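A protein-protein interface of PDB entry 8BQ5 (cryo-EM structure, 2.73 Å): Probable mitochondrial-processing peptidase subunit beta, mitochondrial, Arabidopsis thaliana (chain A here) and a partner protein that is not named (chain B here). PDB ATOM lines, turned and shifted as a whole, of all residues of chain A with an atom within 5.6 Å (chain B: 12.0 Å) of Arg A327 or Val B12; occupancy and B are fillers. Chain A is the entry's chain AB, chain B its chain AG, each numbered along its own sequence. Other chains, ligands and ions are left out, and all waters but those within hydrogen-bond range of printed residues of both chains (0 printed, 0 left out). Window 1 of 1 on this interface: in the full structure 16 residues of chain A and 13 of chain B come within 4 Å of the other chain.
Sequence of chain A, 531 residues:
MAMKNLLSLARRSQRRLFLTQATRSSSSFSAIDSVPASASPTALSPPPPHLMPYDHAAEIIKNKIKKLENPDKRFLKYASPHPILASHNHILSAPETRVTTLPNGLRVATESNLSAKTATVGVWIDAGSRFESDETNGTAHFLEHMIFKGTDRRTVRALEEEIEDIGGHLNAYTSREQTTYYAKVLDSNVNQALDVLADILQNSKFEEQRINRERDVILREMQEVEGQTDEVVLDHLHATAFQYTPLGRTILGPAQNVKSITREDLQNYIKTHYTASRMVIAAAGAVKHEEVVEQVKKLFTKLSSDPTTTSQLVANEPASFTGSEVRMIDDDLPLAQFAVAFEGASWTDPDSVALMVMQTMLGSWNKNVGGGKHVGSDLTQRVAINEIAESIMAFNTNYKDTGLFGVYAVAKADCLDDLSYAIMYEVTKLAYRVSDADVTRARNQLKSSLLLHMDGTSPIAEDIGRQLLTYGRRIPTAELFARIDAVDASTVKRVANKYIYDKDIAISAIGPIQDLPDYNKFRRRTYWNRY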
ATOM      1  N   GLU A 325      10.852 -29.886 -12.886  1.00  0.00           N
ATOM      2  CA  GLU A 325      10.246 -28.995 -13.860  1.00  0.00           C
ATOM      3  C   GLU A 325      11.220 -28.726 -14.996  1.00  0.00           C
ATOM      4  O   GLU A 325      12.439 -28.795 -14.823  1.00  0.00           O
ATOM      5  CB  GLU A 325       9.803 -27.676 -13.217  1.00  0.00           C
ATOM      6  CG  GLU A 325      10.909 -26.655 -13.058  1.00  0.00           C
ATOM      7  CD  GLU A 325      10.516 -25.523 -12.136  1.00  0.00           C
ATOM      8  OE1 GLU A 325      11.396 -25.010 -11.415  1.00  0.00           O
ATOM      9  OE2 GLU A 325       9.326 -25.145 -12.133  1.00  0.00           O
ATOM     10  N   VAL A 326      10.661 -28.432 -16.167  1.00  0.00           N
ATOM     11  CA  VAL A 326      11.422 -27.968 -17.318  1.00  0.00           C
ATOM     12  C   VAL A 326      10.738 -26.719 -17.855  1.00  0.00           C
ATOM     13  O   VAL A 326       9.536 -26.737 -18.140  1.00  0.00           O
ATOM     14  CB  VAL A 326      11.541 -29.051 -18.410  1.00  0.00           C
ATOM     15  CG1 VAL A 326      10.219 -29.781 -18.601  1.00  0.00           C
ATOM     16  CG2 VAL A 326      12.021 -28.443 -19.718  1.00  0.00           C
ATOM     17  N   ARG A 327      11.495 -25.632 -17.969  1.00  0.00           N
ATOM     18  CA  ARG A 327      10.977 -24.342 -18.416  1.00  0.00           C
ATOM     19  C   ARG A 327      11.677 -23.963 -19.711  1.00  0.00           C
ATOM     20  O   ARG A 327      12.887 -23.715 -19.717  1.00  0.00           O
ATOM     21  CB  ARG A 327      11.184 -23.271 -17.348  1.00  0.00           C
ATOM     22  CG  ARG A 327      10.039 -23.156 -16.367  1.00  0.00           C
ATOM     23  CD  ARG A 327      10.494 -22.532 -15.065  1.00  0.00           C
ATOM     24  NE  ARG A 327       9.652 -22.955 -13.953  1.00  0.00           N
ATOM     25  CZ  ARG A 327       8.664 -22.232 -13.443  1.00  0.00           C
ATOM     26  NH1 ARG A 327       8.384 -21.024 -13.901  1.00  0.00           N
ATOM     27  NH2 ARG A 327       7.943 -22.735 -12.445  1.00  0.00           N
ATOM     28  N   MET A 328      10.920 -23.915 -20.803  1.00  0.00           N
ATOM     29  CA  MET A 328      11.452 -23.554 -22.116  1.00  0.00           C
ATOM     30  C   MET A 328      11.089 -22.095 -22.377  1.00  0.00           C
ATOM     31  O   MET A 328      10.034 -21.783 -22.926  1.00  0.00           O
ATOM     32  CB  MET A 328      10.910 -24.483 -23.196  1.00  0.00           C
ATOM     33  CG  MET A 328      11.333 -25.934 -23.026  1.00  0.00           C
ATOM     34  SD  MET A 328      10.222 -27.111 -23.823  1.00  0.00           S
ATOM     35  CE  MET A 328       8.967 -27.310 -22.563  1.00  0.00           C
ATOM     36  N   ILE A 329      11.985 -21.197 -21.982  1.00  0.00           N
ATOM     37  CA  ILE A 329      11.731 -19.764 -22.077  1.00  0.00           C
ATOM     38  C   ILE A 329      11.935 -19.318 -23.519  1.00  0.00           C
ATOM     39  O   ILE A 329      13.016 -19.496 -24.090  1.00  0.00           O
ATOM     40  CB  ILE A 329      12.639 -18.980 -21.122  1.00  0.00           C
ATOM     41  CG1 ILE A 329      12.392 -19.422 -19.678  1.00  0.00           C
ATOM     42  CG2 ILE A 329      12.417 -17.485 -21.278  1.00  0.00           C
ATOM     43  CD1 ILE A 329      13.563 -19.187 -18.760  1.00  0.00           C
ATOM     44  N   ILE A 507       6.157 -29.641 -13.591  1.00  0.00           N
ATOM     45  CA  ILE A 507       5.748 -28.526 -14.434  1.00  0.00           C
ATOM     46  C   ILE A 507       6.545 -28.560 -15.728  1.00  0.00           C
ATOM     47  O   ILE A 507       7.760 -28.778 -15.716  1.00  0.00           O
ATOM     48  CB  ILE A 507       5.930 -27.168 -13.725  1.00  0.00           C
ATOM     49  CG1 ILE A 507       5.303 -27.195 -12.332  1.00  0.00           C
ATOM     50  CG2 ILE A 507       5.352 -26.039 -14.564  1.00  0.00           C
ATOM     51  CD1 ILE A 507       5.888 -26.168 -11.398  1.00  0.00           C
ATOM     52  N   ALA A 509       6.670 -25.952 -19.060  1.00  0.00           N
ATOM     53  CA  ALA A 509       6.184 -24.682 -19.580  1.00  0.00           C
ATOM     54  C   ALA A 509       7.021 -24.250 -20.774  1.00  0.00           C
ATOM     55  O   ALA A 509       8.205 -24.579 -20.875  1.00  0.00           O
ATOM     56  CB  ALA A 509       6.215 -23.592 -18.503  1.00  0.00           C
ATOM     57  N   ILE A 513       7.292 -17.156 -20.317  1.00  0.00           N
ATOM     58  CA  ILE A 513       6.946 -17.706 -19.015  1.00  0.00           C
ATOM     59  C   ILE A 513       7.807 -17.108 -17.904  1.00  0.00           C
ATOM     60  O   ILE A 513       8.029 -17.751 -16.881  1.00  0.00           O
ATOM     61  CB  ILE A 513       7.042 -19.239 -19.027  1.00  0.00           C
ATOM     62  CG1 ILE A 513       8.423 -19.667 -19.529  1.00  0.00           C
ATOM     63  CG2 ILE A 513       5.949 -19.832 -19.894  1.00  0.00           C
ATOM     64  CD1 ILE A 513       8.712 -21.135 -19.360  1.00  0.00           C
ATOM     65  N   LEU A 516       5.721 -16.718 -14.816  1.00  0.00           N
ATOM     66  CA  LEU A 516       5.164 -17.932 -14.238  1.00  0.00           C
ATOM     67  C   LEU A 516       5.826 -18.196 -12.890  1.00  0.00           C
ATOM     68  O   LEU A 516       7.056 -18.119 -12.787  1.00  0.00           O
ATOM     69  CB  LEU A 516       5.372 -19.117 -15.178  1.00  0.00           C
ATOM     70  CG  LEU A 516       4.683 -20.428 -14.798  1.00  0.00           C
ATOM     71  CD1 LEU A 516       3.199 -20.383 -15.123  1.00  0.00           C
ATOM     72  CD2 LEU A 516       5.349 -21.598 -15.495  1.00  0.00           C
ATOM     73  N   PRO A 517       5.057 -18.480 -11.840  1.00  0.00           N
ATOM     74  CA  PRO A 517       5.667 -18.734 -10.530  1.00  0.00           C
ATOM     75  C   PRO A 517       6.633 -19.908 -10.577  1.00  0.00           C
ATOM     76  O   PRO A 517       6.441 -20.875 -11.316  1.00  0.00           O
ATOM     77  CB  PRO A 517       4.463 -19.040  -9.634  1.00  0.00           C
ATOM     78  CG  PRO A 517       3.338 -18.317 -10.264  1.00  0.00           C
ATOM     79  CD  PRO A 517       3.598 -18.311 -11.748  1.00  0.00           C
ATOM     80  N   ASP A 518       7.688 -19.806  -9.778  1.00  0.00           N
ATOM     81  CA  ASP A 518       8.714 -20.832  -9.741  1.00  0.00           C
ATOM     82  C   ASP A 518       8.203 -22.090  -9.039  1.00  0.00           C
ATOM     83  O   ASP A 518       7.051 -22.170  -8.606  1.00  0.00           O
ATOM     84  CB  ASP A 518       9.970 -20.296  -9.060  1.00  0.00           C
ATOM     85  CG  ASP A 518       9.787 -20.095  -7.571  1.00  0.00           C
ATOM     86  OD1 ASP A 518       8.651 -20.216  -7.068  1.00  0.00           O
ATOM     87  OD2 ASP A 518      10.788 -19.810  -6.894  1.00  0.00           O
ATOM     88  N   TYR A 519       9.094 -23.075  -8.905  1.00  0.00           N
ATOM     89  CA  TYR A 519       8.692 -24.358  -8.339  1.00  0.00           C
ATOM     90  C   TYR A 519       8.275 -24.224  -6.880  1.00  0.00           C
ATOM     91  O   TYR A 519       7.304 -24.856  -6.446  1.00  0.00           O
ATOM     92  CB  TYR A 519       9.824 -25.377  -8.483  1.00  0.00           C
ATOM     93  CG  TYR A 519       9.408 -26.793  -8.155  1.00  0.00           C
ATOM     94  CD1 TYR A 519       9.389 -27.249  -6.845  1.00  0.00           C
ATOM     95  CD2 TYR A 519       9.023 -27.671  -9.159  1.00  0.00           C
ATOM     96  CE1 TYR A 519       9.004 -28.535  -6.543  1.00  0.00           C
ATOM     97  CE2 TYR A 519       8.640 -28.961  -8.866  1.00  0.00           C
ATOM     98  CZ  TYR A 519       8.630 -29.388  -7.557  1.00  0.00           C
ATOM     99  OH  TYR A 519       8.247 -30.672  -7.256  1.00  0.00           O
ATOM    100  N   PHE A 522       4.683 -22.946  -6.543  1.00  0.00           N
ATOM    101  CA  PHE A 522       3.726 -24.014  -6.815  1.00  0.00           C
ATOM    102  C   PHE A 522       3.706 -25.039  -5.689  1.00  0.00           C
ATOM    103  O   PHE A 522       2.636 -25.510  -5.286  1.00  0.00           O
ATOM    104  CB  PHE A 522       4.060 -24.695  -8.141  1.00  0.00           C
ATOM    105  CG  PHE A 522       3.500 -23.996  -9.342  1.00  0.00           C
ATOM    106  CD1 PHE A 522       4.252 -23.064 -10.032  1.00  0.00           C
ATOM    107  CD2 PHE A 522       2.226 -24.290  -9.796  1.00  0.00           C
ATOM    108  CE1 PHE A 522       3.739 -22.428 -11.142  1.00  0.00           C
ATOM    109  CE2 PHE A 522       1.710 -23.658 -10.906  1.00  0.00           C
ATOM    110  CZ  PHE A 522       2.468 -22.725 -11.579  1.00  0.00           C
ATOM    111  N   LEU B   8      14.369 -13.343 -23.640  1.00  0.00           N
ATOM    112  CA  LEU B   8      15.371 -14.397 -23.347  1.00  0.00           C
ATOM    113  C   LEU B   8      15.006 -15.712 -24.037  1.00  0.00           C
ATOM    114  O   LEU B   8      13.804 -15.957 -24.239  1.00  0.00           O
ATOM    115  CB  LEU B   8      15.398 -14.563 -21.827  1.00  0.00           C
ATOM    116  CG  LEU B   8      16.391 -15.582 -21.278  1.00  0.00           C
ATOM    117  CD1 LEU B   8      17.812 -15.043 -21.354  1.00  0.00           C
ATOM    118  CD2 LEU B   8      16.027 -15.944 -19.849  1.00  0.00           C
ATOM    119  N   LYS B   9      16.009 -16.512 -24.404  1.00  0.00           N
ATOM    120  CA  LYS B   9      15.761 -17.856 -24.984  1.00  0.00           C
ATOM    121  C   LYS B   9      16.617 -18.851 -24.194  1.00  0.00           C
ATOM    122  O   LYS B   9      17.831 -18.921 -24.466  1.00  0.00           O
ATOM    123  CB  LYS B   9      16.109 -17.876 -26.476  1.00  0.00           C
ATOM    124  CG  LYS B   9      15.907 -19.203 -27.194  1.00  0.00           C
ATOM    125  CD  LYS B   9      14.457 -19.521 -27.466  1.00  0.00           C
ATOM    126  CE  LYS B   9      14.269 -20.609 -28.501  1.00  0.00           C
ATOM    127  NZ  LYS B   9      14.660 -21.942 -27.988  1.00  0.00           N
ATOM    128  N   ALA B  10      16.022 -19.566 -23.236  1.00  0.00           N
ATOM    129  CA  ALA B  10      16.806 -20.562 -22.520  1.00  0.00           C
ATOM    130  C   ALA B  10      15.911 -21.733 -22.149  1.00  0.00           C
ATOM    131  O   ALA B  10      14.682 -21.643 -22.201  1.00  0.00           O
ATOM    132  CB  ALA B  10      17.454 -19.968 -21.265  1.00  0.00           C
ATOM    133  N   VAL B  11      16.550 -22.840 -21.780  1.00  0.00           N
ATOM    134  CA  VAL B  11      15.872 -24.018 -21.250  1.00  0.00           C
ATOM    135  C   VAL B  11      16.447 -24.295 -19.870  1.00  0.00           C
ATOM    136  O   VAL B  11      17.669 -24.418 -19.716  1.00  0.00           O
ATOM    137  CB  VAL B  11      16.035 -25.240 -22.166  1.00  0.00           C
ATOM    138  CG1 VAL B  11      15.215 -26.404 -21.643  1.00  0.00           C
ATOM    139  CG2 VAL B  11      15.631 -24.898 -23.590  1.00  0.00           C
ATOM    140  N   VAL B  12      15.576 -24.394 -18.870  1.00  0.00           N
ATOM    141  CA  VAL B  12      15.984 -24.611 -17.488  1.00  0.00           C
ATOM    142  C   VAL B  12      15.343 -25.894 -16.983  1.00  0.00           C
ATOM    143  O   VAL B  12      14.122 -26.066 -17.082  1.00  0.00           O
ATOM    144  CB  VAL B  12      15.604 -23.424 -16.586  1.00  0.00           C
ATOM    145  CG1 VAL B  12      16.247 -23.578 -15.219  1.00  0.00           C
ATOM    146  CG2 VAL B  12      16.028 -22.114 -17.226  1.00  0.00           C
ATOM    147  N   TYR B  13      16.165 -26.788 -16.444  1.00  0.00           N
ATOM    148  CA  TYR B  13      15.704 -27.989 -15.764  1.00  0.00           C
ATOM    149  C   TYR B  13      15.998 -27.846 -14.280  1.00  0.00           C
ATOM    150  O   TYR B  13      17.111 -27.470 -13.899  1.00  0.00           O
ATOM    151  CB  TYR B  13      16.390 -29.242 -16.310  1.00  0.00           C
ATOM    152  CG  TYR B  13      16.364 -29.377 -17.814  1.00  0.00           C
ATOM    153  CD1 TYR B  13      17.338 -28.779 -18.601  1.00  0.00           C
ATOM    154  CD2 TYR B  13      15.374 -30.117 -18.446  1.00  0.00           C
ATOM    155  CE1 TYR B  13      17.322 -28.904 -19.974  1.00  0.00           C
ATOM    156  CE2 TYR B  13      15.351 -30.249 -19.818  1.00  0.00           C
ATOM    157  CZ  TYR B  13      16.327 -29.641 -20.576  1.00  0.00           C
ATOM    158  OH  TYR B  13      16.306 -29.768 -21.944  1.00  0.00           O
ATOM    159  N   ALA B  14      15.006 -28.140 -13.446  1.00  0.00           N
ATOM    160  CA  ALA B  14      15.158 -28.025 -12.005  1.00  0.00           C
ATOM    161  C   ALA B  14      14.566 -29.252 -11.333  1.00  0.00           C
ATOM    162  O   ALA B  14      13.660 -29.895 -11.865  1.00  0.00           O
ATOM    163  CB  ALA B  14      14.494 -26.752 -11.467  1.00  0.00           C
ATOM    164  N   LEU B  15      15.090 -29.566 -10.154  1.00  0.00           N
ATOM    165  CA  LEU B  15      14.690 -30.738  -9.393  1.00  0.00           C
ATOM    166  C   LEU B  15      14.087 -30.302  -8.065  1.00  0.00           C
ATOM    167  O   LEU B  15      14.460 -29.259  -7.518  1.00  0.00           O
ATOM    168  CB  LEU B  15      15.888 -31.664  -9.161  1.00  0.00           C
ATOM    169  CG  LEU B  15      15.687 -32.968  -8.391  1.00  0.00           C
ATOM    170  CD1 LEU B  15      14.733 -33.888  -9.129  1.00  0.00           C
ATOM    171  CD2 LEU B  15      17.022 -33.652  -8.168  1.00  0.00           C
ATOM    172  N   SER B  16      13.153 -31.099  -7.557  1.00  0.00           N
ATOM    173  CA  SER B  16      12.472 -30.757  -6.318  1.00  0.00           C
ATOM    174  C   SER B  16      13.472 -30.662  -5.168  1.00  0.00           C
ATOM    175  O   SER B  16      14.424 -31.450  -5.106  1.00  0.00           O
ATOM    176  CB  SER B  16      11.404 -31.800  -5.986  1.00  0.00           C
ATOM    177  OG  SER B  16      10.468 -31.293  -5.054  1.00  0.00           O
ATOM    178  N   PRO B  17      13.293 -29.711  -4.249  1.00  0.00           N
ATOM    179  CA  PRO B  17      14.181 -29.649  -3.077  1.00  0.00           C
ATOM    180  C   PRO B  17      14.133 -30.899  -2.221  1.00  0.00           C
ATOM    181  O   PRO B  17      15.110 -31.204  -1.527  1.00  0.00           O
ATOM    182  CB  PRO B  17      13.661 -28.426  -2.309  1.00  0.00           C
ATOM    183  CG  PRO B  17      12.932 -27.615  -3.320  1.00  0.00           C
ATOM    184  CD  PRO B  17      12.341 -28.589  -4.289  1.00  0.00           C
ATOM    185  N   GLN B  20      16.779 -34.011  -3.150  1.00  0.00           N
ATOM    186  CA  GLN B  20      18.209 -33.743  -3.125  1.00  0.00           C
ATOM    187  C   GLN B  20      18.725 -33.757  -1.693  1.00  0.00           C
ATOM    188  O   GLN B  20      17.984 -33.484  -0.746  1.00  0.00           O
ATOM    189  CB  GLN B  20      18.545 -32.386  -3.763  1.00  0.00           C
ATOM    190  CG  GLN B  20      17.601 -31.954  -4.868  1.00  0.00           C
ATOM    191  CD  GLN B  20      17.932 -30.581  -5.412  1.00  0.00           C
ATOM    192  OE1 GLN B  20      19.087 -30.160  -5.401  1.00  0.00           O
ATOM    193  NE2 GLN B  20      16.918 -29.876  -5.895  1.00  0.00           N
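Among the printed residues, 13 pairs touch across the chains.
Of chain B, only Val B12, Tyr B13 and Ala B14 come within 4 Å of Glu A325. Val A326 touches just these residues of chain B: Val B12 (3.3 Å) and Tyr B13 (3.8 Å). Arg A327 touches just these residues of chain B: Ala B10 (3.7 Å), Val B11 (3.4 Å) and Val B12 (2.8 Å). Printed residues of chain B within 4 Å of Met A328: Ala B10 (3.6 Å). Ile A329 touches just these residues of chain B: Leu B8 (3.6 Å), Lys B9 (3.3 Å) and Ala B10 (2.7 Å). Ile A507 touches none of the printed residues of chain B. No residue of chain B comes within 4 Å of Ala A509. No residue of chain B comes within 4 Å of Ile A513. No residue of chain B comes within 4 Å of Leu A516. No residue of chain B comes within 4 Å of Pro A517. Of the printed residues of chain B, Tyr A519 touches Ser B16. Of the printed residues of chain A, Lys B9 touches Ile A329 (3.3 Å). Printed residues of chain A within 4 Å of Ala B10: Arg A327 (3.7 Å), Met A328 (3.6 Å) and Ile A329 (2.7 Å). Printed residues of chain A within 4 Å of Val B11: Arg A327. Of chain A, only Glu A325, Val A326 and Arg A327 come within 4 Å of Val B12. Printed residues of chain A within 4 Å of Ser B16: Tyr A519 (3.2 Å). The nearest residue of chain A that does not touch Val B12 is Ile A329 (4.1 Å). The nearest printed residue of chain A that does not touch Ala B10 is Ile A513 (6.6 Å).
Among the printed residues, merely in contact across the chains: Glu A325 with Val B12 (3.9 Å), Glu A325 with Tyr B13 (3.5 Å), Val A326 with Val B12 (3.3 Å), Val A326 with Tyr B13 (3.8 Å), Arg A327 with Ala B10 (3.7 Å), Arg A327 with Val B11 (3.4 Å), Met A328 with Ala B10 (3.6 Å), Ile A329 with Leu B8 (3.6 Å) and Ile A329 with Lys B9 (3.3 Å).
The backbone carbonyl oxygen (O) of Val A326 sits at hydrogen-bond distance from the backbone NH (N) of Ala A509 (3.1 Å). The guanidinium group (NH2) of Arg A327 lies within salt-bridge range of the side-chain carboxylate (OE2) of Glu A325, 2.8 Å away. The backbone NH of Val A326 lies within hydrogen-bond range of the backbone carbonyl oxygen of Ile A507 (3.0 Å). The backbone NH of Met A328 sits at hydrogen-bond distance from the backbone carbonyl oxygen of Ala A509 (2.8 Å). The backbone carbonyl oxygen of Ser B16 sits at hydrogen-bond distance from the side-chain amide nitrogen of Gln B20 (3.1 Å). The backbone carbonyl oxygen (O) of Leu A516 is in hydrogen-bond range of the guanidinium group (NH1) of Arg A327 (3.4 Å).
The backbone NH (N) of Ile A329 lies within hydrogen-bond range of the backbone carbonyl oxygen (O) of Ala B10 (2.7 Å). N of Ala B14 sits at hydrogen-bond distance from O of Glu A325, at 3.0 Å. The side-chain hydroxyl (OG) of Ser B16 lies within hydrogen-bond range of the side-chain hydroxyl (OH) of Tyr A519 (3.2 Å). The backbone NH (N) of Arg A327 is in hydrogen-bond range of the backbone carbonyl oxygen (O) of Val B12 (2.8 Å).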
